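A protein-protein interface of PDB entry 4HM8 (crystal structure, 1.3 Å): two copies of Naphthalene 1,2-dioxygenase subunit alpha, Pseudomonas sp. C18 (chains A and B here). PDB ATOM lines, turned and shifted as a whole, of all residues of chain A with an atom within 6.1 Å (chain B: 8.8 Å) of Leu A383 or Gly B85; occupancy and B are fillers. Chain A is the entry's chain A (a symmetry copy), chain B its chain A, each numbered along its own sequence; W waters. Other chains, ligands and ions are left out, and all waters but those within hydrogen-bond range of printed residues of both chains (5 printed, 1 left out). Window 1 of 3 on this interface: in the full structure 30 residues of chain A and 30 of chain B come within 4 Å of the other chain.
O of His B83 sits at hydrogen-bond distance from N of Leu A384 (2.8 Å).
The side-chain amide oxygen of Gln A16 lies within hydrogen-bond range of the guanidinium group of Arg B84 (2.8 Å).
The guanidinium group (NH2) of Arg B84 lies within salt-bridge range of the side-chain carboxylate (OE1) of Glu A200, 2.9 Å away.
NH1 of Arg B84 lies within hydrogen-bond range of O of Leu A384, at 2.9 Å.
The backbone carbonyl oxygen (O) of Gly B85 sits at hydrogen-bond distance from the side-chain amide nitrogen (ND2) of Asn A372 (2.9 Å).
The backbone NH of Thr B87 sits at hydrogen-bond distance from the side-chain hydroxyl of Thr A368 (3.1 Å).
The side-chain hydroxyl (OG1) of Thr B87 sits at hydrogen-bond distance from the side-chain amide nitrogen (ND2) of Asn A372.
His A18 touches Gly B85 (CE1 to O, 3.5 Å).
CG of Lys B86 touches OG1 of Thr A368, at 3.4 Å.
Arg B84 touches Ala A369.
Gly B85 touches Ala A369.
Asn A372 touches Val B80.
C of Lys B86 touches ND2 of Asn A372 (3.8 Å).
Arg B84 touches Leu A383.
CD2 of Leu A383 touches N of Gly B85, 3.8 Å away.
Leu A384 touches Arg B82 (CD1 to O, 3.4 Å).
Arg B84 touches Ser A385 (NH1 to CB, 3.7 Å).
Water W3 bridges OH of Tyr B103 and OE2 of Glu A200.
Water W5 bridges the backbone carbonyl oxygen of Asp A382 (2.7 Å) and the backbone carbonyl oxygen of Arg B82 (2.8 Å).
Water W1 lies within hydrogen-bond range of the side-chain carboxylate (OD2) of Asp A382 (2.8 Å) and the guanidinium group (NH2) of Arg B82 (3.3 Å).
Water W4 lies within hydrogen-bond range of the backbone carbonyl oxygen (O) of Asn B79 (2.9 Å) and the side-chain amide oxygen (OD1) of Asn A372 (3.0 Å).
Water W2 lies within hydrogen-bond range of the side-chain carboxylate of Glu A200 (3.0 Å), a ring nitrogen (NE2) of His A21 (3.0 Å) and the backbone carbonyl oxygen of Arg B84 (3.1 Å).
Leu A383 touches three residues of chain B.
Of chain A, only His A18 (3.5 Å), Ala A369 (3.5 Å), Asn A372 (2.9 Å) and Leu A383 (3.8 Å) come within 4 Å of Gly B85.
No residue of chain B comes within 4 Å of Ser A15.
Of chain B, only Arg B84 (3.7 Å) and Gly B85 (3.5 Å) come within 4 Å of Ala A369.
Of the printed residues of chain B, Thr A368 touches Lys B86 and Thr B87.
Printed residues of chain A within 4 Å of Arg B82: Leu A384 (3.4 Å).
Asn B79 touches none of the printed residues of chain A.
Tyr B103 touches none of the printed residues of chain A.
The nearest residue of chain A that does not touch Gly B85 is Thr A368 (4.1 Å).
Of the 16 printed residues of chain B, 8 touch a printed residue of chain A.
Hydrophobic or aromatic side chains of chain B that line the printed part of chain A: Val B80, His B83 and Leu B133.
Of the 19 printed residues of chain A, 10 touch a printed residue of chain B.
Hydrophobic or aromatic side chains of chain A within 4 Å of the printed part of chain B: His A18, Ala A369, Leu A383, Leu A384 and Tyr A417.
Among the printed residues, Asp or Glu carboxylates within 4 Å of a Lys or Arg side-chain nitrogen of the other chain: Glu A200 with Arg B84 (2.9 Å).
No position is printed for both chains.
The backbone NH of Cys B81 sits at hydrogen-bond distance from the backbone carbonyl oxygen of Lys B86, at 2.8 Å.
The backbone carbonyl oxygen (O) of Leu A14 is in hydrogen-bond range of the backbone NH (N) of Ser A385, 2.9 Å away.
N of Leu A383 lies within hydrogen-bond range of O of Gln A16 (2.8 Å).
OG of Ser A385 is in hydrogen-bond range of NE2 of Gln A16, 2.9 Å away.
The side-chain carboxylate of Glu A200 lies within hydrogen-bond range of the side-chain hydroxyl of Tyr A417.
ND2 of Asn A372 sits close to O of Thr A368 (3.2 Å).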
ATOM      1  N   LEU A  14      -3.373   9.778  10.838  1.00  0.00           N
ATOM      2  CA  LEU A  14      -2.876  10.943  10.097  1.00  0.00           C
ATOM      3  C   LEU A  14      -1.381  10.924   9.809  1.00  0.00           C
ATOM      4  O   LEU A  14      -0.916  11.587   8.877  1.00  0.00           O
ATOM      5  CB  LEU A  14      -3.243  12.232  10.831  1.00  0.00           C
ATOM      6  CG  LEU A  14      -4.719  12.576  10.688  1.00  0.00           C
ATOM      7  CD1 LEU A  14      -5.082  13.727  11.602  1.00  0.00           C
ATOM      8  CD2 LEU A  14      -5.029  12.913   9.239  1.00  0.00           C
ATOM      9  N   SER A  15      -0.632  10.179  10.616  1.00  0.00           N
ATOM     10  CA  SER A  15       0.799  10.049  10.416  1.00  0.00           C
ATOM     11  C   SER A  15       1.311   8.780  11.067  1.00  0.00           C
ATOM     12  O   SER A  15       0.636   8.194  11.920  1.00  0.00           O
ATOM     13  CB  SER A  15       1.552  11.265  10.972  1.00  0.00           C
ATOM     14  OG  SER A  15       1.484  11.310  12.392  1.00  0.00           O
ATOM     15  N   GLN A  16       2.498   8.348  10.642  1.00  0.00           N
ATOM     16  CA  GLN A  16       3.162   7.195  11.238  1.00  0.00           C
ATOM     17  C   GLN A  16       4.629   7.516  11.459  1.00  0.00           C
ATOM     18  O   GLN A  16       5.248   8.226  10.660  1.00  0.00           O
ATOM     19  CB  GLN A  16       3.058   5.963  10.327  1.00  0.00           C
ATOM     20  CG  GLN A  16       1.637   5.631   9.850  1.00  0.00           C
ATOM     21  CD  GLN A  16       1.154   6.524   8.715  1.00  0.00           C
ATOM     22  OE1 GLN A  16       1.892   6.800   7.766  1.00  0.00           O
ATOM     23  NE2 GLN A  16      -0.096   6.978   8.804  1.00  0.00           N
ATOM     24  N   LYS A  17       5.197   6.987  12.534  1.00  0.00           N
ATOM     25  CA  LYS A  17       6.635   7.146  12.745  1.00  0.00           C
ATOM     26  C   LYS A  17       7.404   6.380  11.670  1.00  0.00           C
ATOM     27  O   LYS A  17       7.098   5.220  11.377  1.00  0.00           O
ATOM     28  CB  LYS A  17       7.046   6.682  14.146  1.00  0.00           C
ATOM     29  CG  LYS A  17       6.477   7.546  15.271  1.00  0.00           C
ATOM     30  CD  LYS A  17       6.982   8.977  15.125  1.00  0.00           C
ATOM     31  CE  LYS A  17       6.602   9.853  16.302  1.00  0.00           C
ATOM     32  NZ  LYS A  17       7.079  11.261  16.055  1.00  0.00           N
ATOM     33  N   HIS A  18       8.406   7.033  11.087  1.00  0.00           N
ATOM     34  CA  HIS A  18       9.163   6.469   9.973  1.00  0.00           C
ATOM     35  C   HIS A  18       9.856   5.174  10.385  1.00  0.00           C
ATOM     36  O   HIS A  18      10.038   4.274   9.563  1.00  0.00           O
ATOM     37  CB  HIS A  18      10.178   7.502   9.491  1.00  0.00           C
ATOM     38  CG  HIS A  18      10.649   7.301   8.085  1.00  0.00           C
ATOM     39  ND1 HIS A  18      11.259   8.304   7.367  1.00  0.00           N
ATOM     40  CD2 HIS A  18      10.619   6.218   7.269  1.00  0.00           C
ATOM     41  CE1 HIS A  18      11.576   7.857   6.165  1.00  0.00           C
ATOM     42  NE2 HIS A  18      11.204   6.590   6.082  1.00  0.00           N
ATOM     43  N   LEU A  19      10.210   5.049  11.662  1.00  0.00           N
ATOM     44  CA  LEU A  19      10.819   3.810  12.150  1.00  0.00           C
ATOM     45  C   LEU A  19       9.991   2.555  11.867  1.00  0.00           C
ATOM     46  O   LEU A  19      10.534   1.454  11.885  1.00  0.00           O
ATOM     47  CB  LEU A  19      11.122   3.900  13.654  1.00  0.00           C
ATOM     48  CG  LEU A  19       9.913   3.812  14.596  1.00  0.00           C
ATOM     49  CD1 LEU A  19       9.599   2.367  15.011  1.00  0.00           C
ATOM     50  CD2 LEU A  19      10.124   4.682  15.833  1.00  0.00           C
ATOM     51  N   ILE A  20       8.685   2.687  11.634  1.00  0.00           N
ATOM     52  CA  ILE A  20       7.907   1.470  11.386  1.00  0.00           C
ATOM     53  C   ILE A  20       8.392   0.716  10.140  1.00  0.00           C
ATOM     54  O   ILE A  20       8.188  -0.489  10.035  1.00  0.00           O
ATOM     55  CB  ILE A  20       6.371   1.685  11.315  1.00  0.00           C
ATOM     56  CG1 ILE A  20       5.963   2.436  10.043  1.00  0.00           C
ATOM     57  CG2 ILE A  20       5.849   2.340  12.581  1.00  0.00           C
ATOM     58  CD1 ILE A  20       4.449   2.518   9.844  1.00  0.00           C
ATOM     59  N   HIS A  21       9.055   1.406   9.210  1.00  0.00           N
ATOM     60  CA  HIS A  21       9.576   0.729   8.012  1.00  0.00           C
ATOM     61  C   HIS A  21      10.980   0.168   8.211  1.00  0.00           C
ATOM     62  O   HIS A  21      11.502  -0.519   7.329  1.00  0.00           O
ATOM     63  CB  HIS A  21       9.603   1.676   6.805  1.00  0.00           C
ATOM     64  CG  HIS A  21       8.251   2.084   6.316  1.00  0.00           C
ATOM     65  ND1 HIS A  21       7.121   1.312   6.503  1.00  0.00           N
ATOM     66  CD2 HIS A  21       7.844   3.182   5.635  1.00  0.00           C
ATOM     67  CE1 HIS A  21       6.084   1.918   5.961  1.00  0.00           C
ATOM     68  NE2 HIS A  21       6.494   3.057   5.425  1.00  0.00           N
ATOM     69  N   GLU A 200       0.945  -0.322   1.524  1.00  0.00           N
ATOM     70  CA  GLU A 200       0.305   0.992   1.633  1.00  0.00           C
ATOM     71  C   GLU A 200       0.103   1.607   0.251  1.00  0.00           C
ATOM     72  O   GLU A 200      -0.892   2.292   0.001  1.00  0.00           O
ATOM     73  CB  GLU A 200       1.098   1.941   2.552  1.00  0.00           C
ATOM     74  CG  GLU A 200       2.350   2.544   1.895  1.00  0.00           C
ATOM     75  CD  GLU A 200       3.079   3.552   2.766  1.00  0.00           C
ATOM     76  OE1 GLU A 200       3.015   3.433   4.012  1.00  0.00           O
ATOM     77  OE2 GLU A 200       3.719   4.479   2.205  1.00  0.00           O
ATOM     78  N   THR A 368      13.945   3.083  -0.731  1.00  0.00           N
ATOM     79  CA  THR A 368      14.545   4.168   0.045  1.00  0.00           C
ATOM     80  C   THR A 368      13.639   4.663   1.167  1.00  0.00           C
ATOM     81  O   THR A 368      14.133   5.014   2.234  1.00  0.00           O
ATOM     82  CB  THR A 368      15.049   5.361  -0.806  1.00  0.00           C
ATOM     83  OG1 THR A 368      13.943   6.027  -1.423  1.00  0.00           O
ATOM     84  CG2 THR A 368      16.056   4.900  -1.865  1.00  0.00           C
ATOM     85  N   ALA A 369      12.326   4.692   0.945  1.00  0.00           N
ATOM     86  CA  ALA A 369      11.415   5.100   2.012  1.00  0.00           C
ATOM     87  C   ALA A 369      11.571   4.126   3.181  1.00  0.00           C
ATOM     88  O   ALA A 369      11.552   4.531   4.346  1.00  0.00           O
ATOM     89  CB  ALA A 369       9.987   5.120   1.528  1.00  0.00           C
ATOM     90  N   SER A 370      11.743   2.844   2.868  1.00  0.00           N
ATOM     91  CA  SER A 370      11.915   1.833   3.906  1.00  0.00           C
ATOM     92  C   SER A 370      13.250   1.968   4.619  1.00  0.00           C
ATOM     93  O   SER A 370      13.315   1.958   5.851  1.00  0.00           O
ATOM     94  CB  SER A 370      11.788   0.422   3.320  1.00  0.00           C
ATOM     95  OG  SER A 370      10.523   0.223   2.711  1.00  0.00           O
ATOM     96  N   ASN A 372      15.264   4.486   4.806  1.00  0.00           N
ATOM     97  CA  ASN A 372      15.378   5.723   5.568  1.00  0.00           C
ATOM     98  C   ASN A 372      14.806   5.597   6.978  1.00  0.00           C
ATOM     99  O   ASN A 372      15.201   6.339   7.871  1.00  0.00           O
ATOM    100  CB  ASN A 372      14.737   6.897   4.814  1.00  0.00           C
ATOM    101  CG  ASN A 372      15.583   7.364   3.650  1.00  0.00           C
ATOM    102  OD1 ASN A 372      16.794   7.140   3.619  1.00  0.00           O
ATOM    103  ND2 ASN A 372      14.955   8.023   2.694  1.00  0.00           N
ATOM    104  N   SER A 381      10.755  10.665  12.861  1.00  0.00           N
ATOM    105  CA  SER A 381      10.048  11.585  11.973  1.00  0.00           C
ATOM    106  C   SER A 381       8.669  11.050  11.598  1.00  0.00           C
ATOM    107  O   SER A 381       8.380   9.855  11.775  1.00  0.00           O
ATOM    108  CB  SER A 381      10.874  11.858  10.719  1.00  0.00           C
ATOM    109  OG  SER A 381      12.083  12.510  11.072  1.00  0.00           O
ATOM    110  N   ASP A 382       7.819  11.929  11.070  1.00  0.00           N
ATOM    111  CA  ASP A 382       6.429  11.564  10.792  1.00  0.00           C
ATOM    112  C   ASP A 382       6.150  11.452   9.299  1.00  0.00           C
ATOM    113  O   ASP A 382       6.300  12.425   8.555  1.00  0.00           O
ATOM    114  CB  ASP A 382       5.486  12.590  11.427  1.00  0.00           C
ATOM    115  CG  ASP A 382       5.756  12.774  12.903  1.00  0.00           C
ATOM    116  OD1 ASP A 382       5.623  11.780  13.640  1.00  0.00           O
ATOM    117  OD2 ASP A 382       6.110  13.898  13.331  1.00  0.00           O
ATOM    118  N   LEU A 383       5.765  10.254   8.867  1.00  0.00           N
ATOM    119  CA  LEU A 383       5.254  10.032   7.516  1.00  0.00           C
ATOM    120  C   LEU A 383       3.818  10.548   7.484  1.00  0.00           C
ATOM    121  O   LEU A 383       3.022  10.215   8.364  1.00  0.00           O
ATOM    122  CB  LEU A 383       5.254   8.534   7.217  1.00  0.00           C
ATOM    123  CG  LEU A 383       6.606   7.831   7.332  1.00  0.00           C
ATOM    124  CD1 LEU A 383       6.415   6.325   7.294  1.00  0.00           C
ATOM    125  CD2 LEU A 383       7.544   8.295   6.204  1.00  0.00           C
ATOM    126  N   LEU A 384       3.477  11.347   6.478  1.00  0.00           N
ATOM    127  CA  LEU A 384       2.175  12.006   6.439  1.00  0.00           C
ATOM    128  C   LEU A 384       1.150  11.264   5.596  1.00  0.00           C
ATOM    129  O   LEU A 384       1.447  10.841   4.481  1.00  0.00           O
ATOM    130  CB  LEU A 384       2.336  13.405   5.863  1.00  0.00           C
ATOM    131  CG  LEU A 384       3.284  14.311   6.624  1.00  0.00           C
ATOM    132  CD1 LEU A 384       3.355  15.643   5.918  1.00  0.00           C
ATOM    133  CD2 LEU A 384       2.773  14.464   8.043  1.00  0.00           C
ATOM    134  N   SER A 385      -0.061  11.121   6.125  1.00  0.00           N
ATOM    135  CA  SER A 385      -1.174  10.579   5.345  1.00  0.00           C
ATOM    136  C   SER A 385      -2.459  11.345   5.642  1.00  0.00           C
ATOM    137  O   SER A 385      -3.474  10.761   6.024  1.00  0.00           O
ATOM    138  CB  SER A 385      -1.347   9.075   5.580  1.00  0.00           C
ATOM    139  OG  SER A 385      -1.330   8.771   6.957  1.00  0.00           O
ATOM    140  N   TYR A 417      -3.508   2.032   8.547  1.00  0.00           N
ATOM    141  CA  TYR A 417      -2.641   2.253   9.698  1.00  0.00           C
ATOM    142  C   TYR A 417      -3.407   2.310  11.021  1.00  0.00           C
ATOM    143  O   TYR A 417      -2.852   1.988  12.072  1.00  0.00           O
ATOM    144  CB  TYR A 417      -1.709   3.455   9.482  1.00  0.00           C
ATOM    145  CG  TYR A 417      -0.564   3.083   8.568  1.00  0.00           C
ATOM    146  CD1 TYR A 417       0.357   2.115   8.960  1.00  0.00           C
ATOM    147  CD2 TYR A 417      -0.424   3.645   7.299  1.00  0.00           C
ATOM    148  CE1 TYR A 417       1.398   1.732   8.133  1.00  0.00           C
ATOM    149  CE2 TYR A 417       0.630   3.260   6.454  1.00  0.00           C
ATOM    150  CZ  TYR A 417       1.528   2.300   6.880  1.00  0.00           C
ATOM    151  OH  TYR A 417       2.569   1.909   6.063  1.00  0.00           O
ATOM    152  N   ASN B  79      18.268  14.318   3.461  1.00  0.00           N
ATOM    153  CA  ASN B  79      17.899  13.897   2.109  1.00  0.00           C
ATOM    154  C   ASN B  79      16.688  12.969   2.143  1.00  0.00           C
ATOM    155  O   ASN B  79      16.736  11.825   1.679  1.00  0.00           O
ATOM    156  CB  ASN B  79      19.102  13.213   1.451  1.00  0.00           C
ATOM    157  CG  ASN B  79      18.911  12.988  -0.029  1.00  0.00           C
ATOM    158  OD1 ASN B  79      17.996  13.532  -0.645  1.00  0.00           O
ATOM    159  ND2 ASN B  79      19.792  12.190  -0.615  1.00  0.00           N
ATOM    160  N   VAL B  80      15.594  13.469   2.715  1.00  0.00           N
ATOM    161  CA  VAL B  80      14.411  12.660   3.007  1.00  0.00           C
ATOM    162  C   VAL B  80      13.171  13.516   2.795  1.00  0.00           C
ATOM    163  O   VAL B  80      13.034  14.593   3.391  1.00  0.00           O
ATOM    164  CB  VAL B  80      14.411  12.141   4.474  1.00  0.00           C
ATOM    165  CG1 VAL B  80      13.174  11.287   4.749  1.00  0.00           C
ATOM    166  CG2 VAL B  80      15.679  11.338   4.792  1.00  0.00           C
ATOM    167  N   CYS B  81      12.271  13.044   1.942  1.00  0.00           N
ATOM    168  CA  CYS B  81      11.048  13.774   1.643  1.00  0.00           C
ATOM    169  C   CYS B  81      10.116  13.860   2.857  1.00  0.00           C
ATOM    170  O   CYS B  81       9.928  12.867   3.568  1.00  0.00           O
ATOM    171  CB  CYS B  81      10.313  13.104   0.485  1.00  0.00           C
ATOM    172  SG  CYS B  81       8.848  14.007  -0.014  1.00  0.00           S
ATOM    173  N   ARG B  82       9.515  15.032   3.068  1.00  0.00           N
ATOM    174  CA  ARG B  82       8.645  15.275   4.223  1.00  0.00           C
ATOM    175  C   ARG B  82       7.266  14.631   4.094  1.00  0.00           C
ATOM    176  O   ARG B  82       6.468  14.657   5.035  1.00  0.00           O
ATOM    177  CB  ARG B  82       8.476  16.786   4.475  1.00  0.00           C
ATOM    178  CG  ARG B  82       9.707  17.495   5.066  1.00  0.00           C
ATOM    179  CD  ARG B  82      10.088  16.963   6.455  1.00  0.00           C
ATOM    180  NE  ARG B  82       8.944  16.858   7.362  1.00  0.00           N
ATOM    181  CZ  ARG B  82       8.467  17.861   8.101  1.00  0.00           C
ATOM    182  NH1 ARG B  82       9.019  19.072   8.038  1.00  0.00           N
ATOM    183  NH2 ARG B  82       7.418  17.659   8.889  1.00  0.00           N
ATOM    184  N   HIS B  83       6.971  14.063   2.933  1.00  0.00           N
ATOM    185  CA  HIS B  83       5.670  13.434   2.730  1.00  0.00           C
ATOM    186  C   HIS B  83       5.732  12.000   3.255  1.00  0.00           C
ATOM    187  O   HIS B  83       5.333  11.727   4.389  1.00  0.00           O
ATOM    188  CB  HIS B  83       5.261  13.489   1.252  1.00  0.00           C
ATOM    189  CG  HIS B  83       3.953  12.818   0.950  1.00  0.00           C
ATOM    190  ND1 HIS B  83       3.764  12.022  -0.164  1.00  0.00           N
ATOM    191  CD2 HIS B  83       2.757  12.846   1.587  1.00  0.00           C
ATOM    192  CE1 HIS B  83       2.525  11.572  -0.189  1.00  0.00           C
ATOM    193  NE2 HIS B  83       1.889  12.058   0.865  1.00  0.00           N
ATOM    194  N   ARG B  84       6.260  11.079   2.457  1.00  0.00           N
ATOM    195  CA  ARG B  84       6.376   9.702   2.921  1.00  0.00           C
ATOM    196  C   ARG B  84       7.782   9.110   2.907  1.00  0.00           C
ATOM    197  O   ARG B  84       7.963   7.891   2.835  1.00  0.00           O
ATOM    198  CB  ARG B  84       5.329   8.822   2.247  1.00  0.00           C
ATOM    199  CG  ARG B  84       3.922   9.328   2.628  1.00  0.00           C
ATOM    200  CD  ARG B  84       2.844   8.306   2.498  1.00  0.00           C
ATOM    201  NE  ARG B  84       3.077   7.154   3.353  1.00  0.00           N
ATOM    202  CZ  ARG B  84       2.761   7.092   4.645  1.00  0.00           C
ATOM    203  NH1 ARG B  84       2.228   8.141   5.268  1.00  0.00           N
ATOM    204  NH2 ARG B  84       2.990   5.974   5.323  1.00  0.00           N
ATOM    205  N   GLY B  85       8.774   9.989   3.019  1.00  0.00           N
ATOM    206  CA  GLY B  85      10.096   9.587   3.458  1.00  0.00           C
ATOM    207  C   GLY B  85      11.038   9.047   2.413  1.00  0.00           C
ATOM    208  O   GLY B  85      12.068   8.460   2.758  1.00  0.00           O
ATOM    209  N   LYS B  86      10.708   9.256   1.142  1.00  0.00           N
ATOM    210  CA  LYS B  86      11.558   8.802   0.046  1.00  0.00           C
ATOM    211  C   LYS B  86      12.859   9.614  -0.019  1.00  0.00           C
ATOM    212  O   LYS B  86      12.893  10.781   0.356  1.00  0.00           O
ATOM    213  CB  LYS B  86      10.782   8.916  -1.270  1.00  0.00           C
ATOM    214  CG  LYS B  86      11.344   8.074  -2.384  1.00  0.00           C
ATOM    215  CD  LYS B  86      12.004   8.929  -3.420  1.00  0.00           C
ATOM    216  CE  LYS B  86      12.928   8.091  -4.276  1.00  0.00           C
ATOM    217  NZ  LYS B  86      13.775   8.958  -5.137  1.00  0.00           N
ATOM    218  N   THR B  87      13.940   8.997  -0.477  1.00  0.00           N
ATOM    219  CA  THR B  87      15.187   9.744  -0.648  1.00  0.00           C
ATOM    220  C   THR B  87      15.055  10.741  -1.794  1.00  0.00           C
ATOM    221  O   THR B  87      14.733  10.373  -2.920  1.00  0.00           O
ATOM    222  CB  THR B  87      16.370   8.801  -0.896  1.00  0.00           C
ATOM    223  OG1 THR B  87      16.594   8.041   0.293  1.00  0.00           O
ATOM    224  CG2 THR B  87      17.640   9.579  -1.240  1.00  0.00           C
ATOM    225  N   LEU B  88      15.317  12.008  -1.507  1.00  0.00           N
ATOM    226  CA  LEU B  88      15.045  13.076  -2.470  1.00  0.00           C
ATOM    227  C   LEU B  88      16.047  13.079  -3.628  1.00  0.00           C
ATOM    228  O   LEU B  88      15.664  13.075  -4.806  1.00  0.00           O
ATOM    229  CB  LEU B  88      15.081  14.413  -1.743  1.00  0.00           C
ATOM    230  CG  LEU B  88      14.075  15.493  -2.083  1.00  0.00           C
ATOM    231  CD1 LEU B  88      12.657  14.930  -2.180  1.00  0.00           C
ATOM    232  CD2 LEU B  88      14.162  16.555  -0.996  1.00  0.00           C
ATOM    233  N   CYS B 101      10.620  15.265  -5.512  1.00  0.00           N
ATOM    234  CA  CYS B 101      10.534  13.870  -5.108  1.00  0.00           C
ATOM    235  C   CYS B 101       9.925  12.994  -6.207  1.00  0.00           C
ATOM    236  O   CYS B 101       8.857  13.317  -6.744  1.00  0.00           O
ATOM    237  CB  CYS B 101       9.705  13.753  -3.839  1.00  0.00           C
ATOM    238  SG  CYS B 101       9.669  12.081  -3.198  1.00  0.00           S
ATOM    239  N   TYR B 103       8.458  10.215  -5.947  1.00  0.00           N
ATOM    240  CA  TYR B 103       7.307   9.420  -5.529  1.00  0.00           C
ATOM    241  C   TYR B 103       5.991  10.137  -5.884  1.00  0.00           C
ATOM    242  O   TYR B 103       5.278   9.708  -6.798  1.00  0.00           O
ATOM    243  CB  TYR B 103       7.430   9.079  -4.037  1.00  0.00           C
ATOM    244  CG  TYR B 103       6.643   7.865  -3.572  1.00  0.00           C
ATOM    245  CD1 TYR B 103       5.620   7.318  -4.348  1.00  0.00           C
ATOM    246  CD2 TYR B 103       6.909   7.280  -2.337  1.00  0.00           C
ATOM    247  CE1 TYR B 103       4.894   6.220  -3.912  1.00  0.00           C
ATOM    248  CE2 TYR B 103       6.186   6.180  -1.891  1.00  0.00           C
ATOM    249  CZ  TYR B 103       5.182   5.657  -2.687  1.00  0.00           C
ATOM    250  OH  TYR B 103       4.467   4.569  -2.242  1.00  0.00           O
ATOM    251  N   HIS B 104       5.687  11.241  -5.200  1.00  0.00           N
ATOM    252  CA  HIS B 104       4.467  12.001  -5.486  1.00  0.00           C
ATOM    253  C   HIS B 104       4.749  13.418  -5.981  1.00  0.00           C
ATOM    254  O   HIS B 104       3.837  14.230  -6.094  1.00  0.00           O
ATOM    255  CB  HIS B 104       3.527  12.044  -4.271  1.00  0.00           C
ATOM    256  CG  HIS B 104       3.316  10.710  -3.619  1.00  0.00           C
ATOM    257  ND1 HIS B 104       4.172  10.202  -2.666  1.00  0.00           N
ATOM    258  CD2 HIS B 104       2.349   9.777  -3.781  1.00  0.00           C
ATOM    259  CE1 HIS B 104       3.743   9.020  -2.264  1.00  0.00           C
ATOM    260  NE2 HIS B 104       2.642   8.736  -2.932  1.00  0.00           N
ATOM    261  N   TRP B 106       6.447  16.123  -4.878  1.00  0.00           N
ATOM    262  CA  TRP B 106       6.629  17.324  -4.053  1.00  0.00           C
ATOM    263  C   TRP B 106       7.947  18.015  -4.391  1.00  0.00           C
ATOM    264  O   TRP B 106       8.971  17.356  -4.603  1.00  0.00           O
ATOM    265  CB  TRP B 106       6.602  16.999  -2.560  1.00  0.00           C
ATOM    266  CG  TRP B 106       5.247  16.683  -1.994  1.00  0.00           C
ATOM    267  CD1 TRP B 106       4.147  16.248  -2.670  1.00  0.00           C
ATOM    268  CD2 TRP B 106       4.866  16.769  -0.617  1.00  0.00           C
ATOM    269  NE1 TRP B 106       3.100  16.066  -1.796  1.00  0.00           N
ATOM    270  CE2 TRP B 106       3.517  16.375  -0.527  1.00  0.00           C
ATOM    271  CE3 TRP B 106       5.538  17.150   0.552  1.00  0.00           C
ATOM    272  CZ2 TRP B 106       2.821  16.347   0.688  1.00  0.00           C
ATOM    273  CZ3 TRP B 106       4.851  17.110   1.762  1.00  0.00           C
ATOM    274  CH2 TRP B 106       3.503  16.720   1.816  1.00  0.00           C
ATOM    275  N   PHE B 108      10.869  20.755  -3.372  1.00  0.00           N
ATOM    276  CA  PHE B 108      11.522  21.509  -2.311  1.00  0.00           C
ATOM    277  C   PHE B 108      12.548  22.449  -2.916  1.00  0.00           C
ATOM    278  O   PHE B 108      13.210  22.109  -3.902  1.00  0.00           O
ATOM    279  CB  PHE B 108      12.207  20.559  -1.321  1.00  0.00           C
ATOM    280  CG  PHE B 108      11.252  19.633  -0.615  1.00  0.00           C
ATOM    281  CD1 PHE B 108      10.660  20.008   0.586  1.00  0.00           C
ATOM    282  CD2 PHE B 108      10.940  18.390  -1.154  1.00  0.00           C
ATOM    283  CE1 PHE B 108       9.773  19.160   1.239  1.00  0.00           C
ATOM    284  CE2 PHE B 108      10.046  17.531  -0.508  1.00  0.00           C
ATOM    285  CZ  PHE B 108       9.461  17.922   0.689  1.00  0.00           C
ATOM    286  N   LEU B 133       6.455  22.186   6.564  1.00  0.00           N
ATOM    287  CA  LEU B 133       6.869  20.970   5.871  1.00  0.00           C
ATOM    288  C   LEU B 133       8.183  21.116   5.112  1.00  0.00           C
ATOM    289  O   LEU B 133       8.437  20.387   4.149  1.00  0.00           O
ATOM    290  CB  LEU B 133       5.758  20.493   4.936  1.00  0.00           C
ATOM    291  CG  LEU B 133       4.510  19.961   5.638  1.00  0.00           C
ATOM    292  CD1 LEU B 133       3.403  19.656   4.645  1.00  0.00           C
ATOM    293  CD2 LEU B 133       4.877  18.728   6.418  1.00  0.00           C
HETATM  294  O   HOH W   1       6.707  16.009  11.643  1.00  0.00           O
HETATM  295  O   HOH W   2       6.224   5.361   3.538  1.00  0.00           O
HETATM  296  O   HOH W   3       5.118   3.146  -0.040  1.00  0.00           O
HETATM  297  O   HOH W   4      18.298   9.701   2.966  1.00  0.00           O
HETATM  298  O   HOH W   5       6.545  15.008   7.768  1.00  0.00           O
